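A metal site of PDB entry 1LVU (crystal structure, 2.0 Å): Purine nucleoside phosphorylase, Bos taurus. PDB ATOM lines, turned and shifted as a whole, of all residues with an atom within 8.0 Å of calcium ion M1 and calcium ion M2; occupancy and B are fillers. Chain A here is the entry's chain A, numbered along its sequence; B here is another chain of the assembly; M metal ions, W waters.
Calcium ion M1 is bound by OE2 of Glu 58 of chain A (2.2 Å), water W5 (2.3 Å), O of Ser 51 of chain A (2.4 Å), water W2 (2.4 Å), OE2 of Glu 58 of chain B (2.4 Å), water W6 (2.5 Å) and OE1 of Glu 58 of chain B (2.5 Å). Calcium ion M1 has seven donor atoms within binding distance.
Calcium ion M2 is bound by the side-chain carboxylate (OE1) of Glu 58 of chain B (2.1 Å). Water W3 binds calcium ion M2. O of Ser 51 of chain B binds calcium ion M2, at 2.4 Å. Calcium ion M2 is bound by water W4 (2.4 Å). Calcium ion M2 is bound by water W1 (2.4 Å). The side-chain carboxylate (OE1) of Glu 58 of chain A binds calcium ion M2 (2.4 Å). The side-chain carboxylate (OE2) of Glu 58 of chain A binds calcium ion M2 (2.5 Å). Calcium ion M2 has seven donor atoms within binding distance.
Of the 21 residues printed, 3 come within 4 Å of calcium ion M1. The nearest printed residue that does not touch calcium ion M1 is Ser 51 of chain B (4.3 Å).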
ATOM      1  N   ASP A  49       7.982  15.539  17.658  1.00  0.00           N
ATOM      2  CA  ASP A  49       9.081  16.415  18.062  1.00  0.00           C
ATOM      3  C   ASP A  49      10.278  15.991  17.227  1.00  0.00           C
ATOM      4  O   ASP A  49      10.465  14.797  16.964  1.00  0.00           O
ATOM      5  CB  ASP A  49       9.405  16.244  19.543  1.00  0.00           C
ATOM      6  CG  ASP A  49       8.289  16.710  20.448  1.00  0.00           C
ATOM      7  OD1 ASP A  49       7.737  17.813  20.217  1.00  0.00           O
ATOM      8  OD2 ASP A  49       7.964  15.975  21.401  1.00  0.00           O
ATOM      9  N   TYR A  50      11.089  16.955  16.800  1.00  0.00           N
ATOM     10  CA  TYR A  50      12.267  16.662  16.000  1.00  0.00           C
ATOM     11  C   TYR A  50      13.132  15.639  16.724  1.00  0.00           C
ATOM     12  O   TYR A  50      13.648  14.691  16.122  1.00  0.00           O
ATOM     13  CB  TYR A  50      13.108  17.915  15.764  1.00  0.00           C
ATOM     14  CG  TYR A  50      12.486  18.991  14.895  1.00  0.00           C
ATOM     15  CD1 TYR A  50      11.461  18.684  14.003  1.00  0.00           C
ATOM     16  CD2 TYR A  50      12.955  20.302  14.934  1.00  0.00           C
ATOM     17  CE1 TYR A  50      10.918  19.667  13.171  1.00  0.00           C
ATOM     18  CE2 TYR A  50      12.423  21.282  14.111  1.00  0.00           C
ATOM     19  CZ  TYR A  50      11.409  20.962  13.234  1.00  0.00           C
ATOM     20  OH  TYR A  50      10.885  21.946  12.414  1.00  0.00           O
ATOM     21  N   SER A  51      13.272  15.835  18.027  1.00  0.00           N
ATOM     22  CA  SER A  51      14.093  14.973  18.872  1.00  0.00           C
ATOM     23  C   SER A  51      13.759  13.479  18.810  1.00  0.00           C
ATOM     24  O   SER A  51      14.637  12.647  18.951  1.00  0.00           O
ATOM     25  CB  SER A  51      14.016  15.455  20.336  1.00  0.00           C
ATOM     26  OG  SER A  51      12.695  15.424  20.824  1.00  0.00           O
ATOM     27  N   GLU A  52      12.488  13.139  18.591  1.00  0.00           N
ATOM     28  CA  GLU A  52      12.102  11.722  18.533  1.00  0.00           C
ATOM     29  C   GLU A  52      12.216  11.110  17.138  1.00  0.00           C
ATOM     30  O   GLU A  52      12.234   9.875  16.996  1.00  0.00           O
ATOM     31  CB  GLU A  52      10.668  11.526  19.036  1.00  0.00           C
ATOM     32  CG  GLU A  52       9.615  12.224  18.208  1.00  0.00           C
ATOM     33  CD  GLU A  52       8.208  11.984  18.727  1.00  0.00           C
ATOM     34  OE1 GLU A  52       7.401  12.949  18.719  1.00  0.00           O
ATOM     35  OE2 GLU A  52       7.903  10.849  19.135  1.00  0.00           O
ATOM     36  N   ILE A  53      12.281  11.948  16.115  1.00  0.00           N
ATOM     37  CA  ILE A  53      12.384  11.467  14.733  1.00  0.00           C
ATOM     38  C   ILE A  53      13.806  11.000  14.439  1.00  0.00           C
ATOM     39  O   ILE A  53      14.762  11.753  14.606  1.00  0.00           O
ATOM     40  CB  ILE A  53      12.036  12.580  13.721  1.00  0.00           C
ATOM     41  CG1 ILE A  53      10.662  13.182  14.051  1.00  0.00           C
ATOM     42  CG2 ILE A  53      12.030  12.011  12.302  1.00  0.00           C
ATOM     43  CD1 ILE A  53      10.288  14.362  13.144  1.00  0.00           C
ATOM     44  N   PRO A  54      13.961   9.741  14.006  1.00  0.00           N
ATOM     45  CA  PRO A  54      15.282   9.204  13.698  1.00  0.00           C
ATOM     46  C   PRO A  54      16.074  10.065  12.721  1.00  0.00           C
ATOM     47  O   PRO A  54      15.541  10.527  11.707  1.00  0.00           O
ATOM     48  CB  PRO A  54      14.956   7.824  13.104  1.00  0.00           C
ATOM     49  CG  PRO A  54      13.720   7.438  13.857  1.00  0.00           C
ATOM     50  CD  PRO A  54      12.915   8.718  13.836  1.00  0.00           C
ATOM     51  N   ASN A  55      17.348  10.292  13.044  1.00  0.00           N
ATOM     52  CA  ASN A  55      18.285  11.079  12.217  1.00  0.00           C
ATOM     53  C   ASN A  55      18.042  12.575  12.146  1.00  0.00           C
ATOM     54  O   ASN A  55      18.880  13.313  11.636  1.00  0.00           O
ATOM     55  CB  ASN A  55      18.341  10.503  10.803  1.00  0.00           C
ATOM     56  CG  ASN A  55      18.811   9.077  10.775  1.00  0.00           C
ATOM     57  OD1 ASN A  55      19.800   8.740  11.430  1.00  0.00           O
ATOM     58  ND2 ASN A  55      18.121   8.223  10.022  1.00  0.00           N
ATOM     59  N   PHE A  56      16.910  13.031  12.651  1.00  0.00           N
ATOM     60  CA  PHE A  56      16.574  14.452  12.611  1.00  0.00           C
ATOM     61  C   PHE A  56      17.487  15.314  13.481  1.00  0.00           C
ATOM     62  O   PHE A  56      17.854  14.925  14.583  1.00  0.00           O
ATOM     63  CB  PHE A  56      15.136  14.669  13.084  1.00  0.00           C
ATOM     64  CG  PHE A  56      14.261  15.324  12.067  1.00  0.00           C
ATOM     65  CD1 PHE A  56      13.787  14.614  10.970  1.00  0.00           C
ATOM     66  CD2 PHE A  56      13.887  16.655  12.211  1.00  0.00           C
ATOM     67  CE1 PHE A  56      12.952  15.222  10.031  1.00  0.00           C
ATOM     68  CE2 PHE A  56      13.055  17.271  11.283  1.00  0.00           C
ATOM     69  CZ  PHE A  56      12.585  16.545  10.197  1.00  0.00           C
ATOM     70  N   PRO A  57      17.890  16.481  12.962  1.00  0.00           N
ATOM     71  CA  PRO A  57      18.751  17.337  13.788  1.00  0.00           C
ATOM     72  C   PRO A  57      17.868  17.838  14.933  1.00  0.00           C
ATOM     73  O   PRO A  57      16.651  17.899  14.793  1.00  0.00           O
ATOM     74  CB  PRO A  57      19.132  18.465  12.828  1.00  0.00           C
ATOM     75  CG  PRO A  57      19.132  17.767  11.471  1.00  0.00           C
ATOM     76  CD  PRO A  57      17.885  16.925  11.556  1.00  0.00           C
ATOM     77  N   GLU A  58      18.470  18.198  16.056  1.00  0.00           N
ATOM     78  CA  GLU A  58      17.691  18.695  17.181  1.00  0.00           C
ATOM     79  C   GLU A  58      17.912  20.179  17.423  1.00  0.00           C
ATOM     80  O   GLU A  58      19.028  20.675  17.295  1.00  0.00           O
ATOM     81  CB  GLU A  58      17.991  17.867  18.439  1.00  0.00           C
ATOM     82  CG  GLU A  58      17.210  16.559  18.468  1.00  0.00           C
ATOM     83  CD  GLU A  58      17.511  15.685  19.661  1.00  0.00           C
ATOM     84  OE1 GLU A  58      17.808  16.243  20.738  1.00  0.00           O
ATOM     85  OE2 GLU A  58      17.433  14.453  19.519  1.00  0.00           O
ATOM     86  N   ASP B  49      11.047  10.556  27.320  1.00  0.00           N
ATOM     87  CA  ASP B  49      11.807   9.731  26.389  1.00  0.00           C
ATOM     88  C   ASP B  49      13.247  10.237  26.418  1.00  0.00           C
ATOM     89  O   ASP B  49      13.472  11.444  26.459  1.00  0.00           O
ATOM     90  CB  ASP B  49      11.276   9.853  24.956  1.00  0.00           C
ATOM     91  CG  ASP B  49       9.853   9.349  24.819  1.00  0.00           C
ATOM     92  OD1 ASP B  49       9.566   8.236  25.305  1.00  0.00           O
ATOM     93  OD2 ASP B  49       9.026  10.064  24.209  1.00  0.00           O
ATOM     94  N   TYR B  50      14.214   9.334  26.393  1.00  0.00           N
ATOM     95  CA  TYR B  50      15.621   9.750  26.410  1.00  0.00           C
ATOM     96  C   TYR B  50      15.895  10.793  25.347  1.00  0.00           C
ATOM     97  O   TYR B  50      16.643  11.746  25.582  1.00  0.00           O
ATOM     98  CB  TYR B  50      16.547   8.557  26.160  1.00  0.00           C
ATOM     99  CG  TYR B  50      16.549   7.508  27.250  1.00  0.00           C
ATOM    100  CD1 TYR B  50      16.186   7.831  28.560  1.00  0.00           C
ATOM    101  CD2 TYR B  50      16.987   6.217  26.982  1.00  0.00           C
ATOM    102  CE1 TYR B  50      16.244   6.875  29.571  1.00  0.00           C
ATOM    103  CE2 TYR B  50      17.050   5.257  27.985  1.00  0.00           C
ATOM    104  CZ  TYR B  50      16.675   5.592  29.280  1.00  0.00           C
ATOM    105  OH  TYR B  50      16.739   4.643  30.264  1.00  0.00           O
ATOM    106  N   SER B  51      15.293  10.612  24.178  1.00  0.00           N
ATOM    107  CA  SER B  51      15.489  11.523  23.057  1.00  0.00           C
ATOM    108  C   SER B  51      15.141  12.986  23.330  1.00  0.00           C
ATOM    109  O   SER B  51      15.716  13.880  22.719  1.00  0.00           O
ATOM    110  CB  SER B  51      14.690  11.033  21.848  1.00  0.00           C
ATOM    111  OG  SER B  51      13.311  10.949  22.155  1.00  0.00           O
ATOM    112  N   GLU B  52      14.205  13.233  24.236  1.00  0.00           N
ATOM    113  CA  GLU B  52      13.811  14.611  24.525  1.00  0.00           C
ATOM    114  C   GLU B  52      14.596  15.271  25.645  1.00  0.00           C
ATOM    115  O   GLU B  52      14.511  16.486  25.833  1.00  0.00           O
ATOM    116  CB  GLU B  52      12.319  14.690  24.854  1.00  0.00           C
ATOM    117  CG  GLU B  52      11.905  13.888  26.060  1.00  0.00           C
ATOM    118  CD  GLU B  52      10.425  14.024  26.378  1.00  0.00           C
ATOM    119  OE1 GLU B  52       9.783  12.994  26.637  1.00  0.00           O
ATOM    120  OE2 GLU B  52       9.921  15.167  26.367  1.00  0.00           O
ATOM    121  N   ILE B  53      15.353  14.484  26.406  1.00  0.00           N
ATOM    122  CA  ILE B  53      16.130  15.037  27.500  1.00  0.00           C
ATOM    123  C   ILE B  53      17.443  15.619  26.968  1.00  0.00           C
ATOM    124  O   ILE B  53      18.205  14.922  26.325  1.00  0.00           O
ATOM    125  CB  ILE B  53      16.455  13.961  28.555  1.00  0.00           C
ATOM    126  CG1 ILE B  53      15.164  13.306  29.062  1.00  0.00           C
ATOM    127  CG2 ILE B  53      17.195  14.581  29.720  1.00  0.00           C
ATOM    128  CD1 ILE B  53      15.397  12.104  29.967  1.00  0.00           C
ATOM    129  N   PRO B  54      17.693  16.911  27.229  1.00  0.00           N
ATOM    130  CA  PRO B  54      18.929  17.555  26.757  1.00  0.00           C
ATOM    131  C   PRO B  54      20.199  16.792  27.172  1.00  0.00           C
ATOM    132  O   PRO B  54      20.313  16.352  28.319  1.00  0.00           O
ATOM    133  CB  PRO B  54      18.865  18.936  27.408  1.00  0.00           C
ATOM    134  CG  PRO B  54      17.388  19.212  27.480  1.00  0.00           C
ATOM    135  CD  PRO B  54      16.825  17.867  27.937  1.00  0.00           C
ATOM    136  N   ASN B  55      21.122  16.625  26.226  1.00  0.00           N
ATOM    137  CA  ASN B  55      22.400  15.945  26.455  1.00  0.00           C
ATOM    138  C   ASN B  55      22.323  14.436  26.664  1.00  0.00           C
ATOM    139  O   ASN B  55      23.348  13.782  26.870  1.00  0.00           O
ATOM    140  CB  ASN B  55      23.129  16.561  27.655  1.00  0.00           C
ATOM    141  CG  ASN B  55      23.349  18.050  27.498  1.00  0.00           C
ATOM    142  OD1 ASN B  55      23.759  18.507  26.438  1.00  0.00           O
ATOM    143  ND2 ASN B  55      23.097  18.803  28.553  1.00  0.00           N
ATOM    144  N   PHE B  56      21.119  13.879  26.609  1.00  0.00           N
ATOM    145  CA  PHE B  56      20.941  12.480  27.060  1.00  0.00           C
ATOM    146  C   PHE B  56      21.261  11.663  25.821  1.00  0.00           C
ATOM    147  O   PHE B  56      20.870  12.031  24.715  1.00  0.00           O
ATOM    148  CB  PHE B  56      19.499  12.205  27.470  1.00  0.00           C
ATOM    149  CG  PHE B  56      19.354  11.526  28.801  1.00  0.00           C
ATOM    150  CD1 PHE B  56      19.607  12.215  29.975  1.00  0.00           C
ATOM    151  CD2 PHE B  56      18.971  10.197  28.868  1.00  0.00           C
ATOM    152  CE1 PHE B  56      19.471  11.588  31.217  1.00  0.00           C
ATOM    153  CE2 PHE B  56      18.831   9.561  30.099  1.00  0.00           C
ATOM    154  CZ  PHE B  56      19.082  10.259  31.267  1.00  0.00           C
ATOM    155  N   PRO B  57      21.990  10.549  25.978  1.00  0.00           N
ATOM    156  CA  PRO B  57      22.294   9.737  24.805  1.00  0.00           C
ATOM    157  C   PRO B  57      20.956   9.169  24.350  1.00  0.00           C
ATOM    158  O   PRO B  57      20.010   9.128  25.131  1.00  0.00           O
ATOM    159  CB  PRO B  57      23.209   8.646  25.362  1.00  0.00           C
ATOM    160  CG  PRO B  57      23.912   9.339  26.502  1.00  0.00           C
ATOM    161  CD  PRO B  57      22.764  10.099  27.145  1.00  0.00           C
ATOM    162  N   GLU B  58      20.868   8.732  23.095  1.00  0.00           N
ATOM    163  CA  GLU B  58      19.615   8.168  22.601  1.00  0.00           C
ATOM    164  C   GLU B  58      19.816   6.710  22.242  1.00  0.00           C
ATOM    165  O   GLU B  58      20.884   6.316  21.793  1.00  0.00           O
ATOM    166  CB  GLU B  58      19.106   8.954  21.386  1.00  0.00           C
ATOM    167  CG  GLU B  58      18.813  10.406  21.714  1.00  0.00           C
ATOM    168  CD  GLU B  58      18.053  11.131  20.617  1.00  0.00           C
ATOM    169  OE1 GLU B  58      17.768  12.340  20.807  1.00  0.00           O
ATOM    170  OE2 GLU B  58      17.738  10.508  19.577  1.00  0.00           O
ATOM    171  N   SER B  59      18.770   5.926  22.468  1.00  0.00           N
ATOM    172  CA  SER B  59      18.771   4.489  22.202  1.00  0.00           C
ATOM    173  C   SER B  59      19.243   4.144  20.791  1.00  0.00           C
ATOM    174  O   SER B  59      19.157   4.963  19.877  1.00  0.00           O
ATOM    175  CB  SER B  59      17.370   3.914  22.434  1.00  0.00           C
ATOM    176  OG  SER B  59      16.864   4.353  23.691  1.00  0.00           O
HETATM  177 CA    CA M   1      16.944  12.535  18.455  1.00  0.00          CA
HETATM  178 CA    CA M   2      17.940  14.127  21.945  1.00  0.00          CA
HETATM  179  O   HOH W   1      18.436  12.804  23.907  1.00  0.00           O
HETATM  180  O   HOH W   2      16.324  10.949  16.753  1.00  0.00           O
HETATM  181  O   HOH W   3      18.244  15.643  23.543  1.00  0.00           O
HETATM  182  O   HOH W   4      20.269  14.047  21.380  1.00  0.00           O
HETATM  183  O   HOH W   5      19.042  12.978  17.754  1.00  0.00           O
HETATM  184  O   HOH W   6      16.290  13.917  16.487  1.00  0.00           O
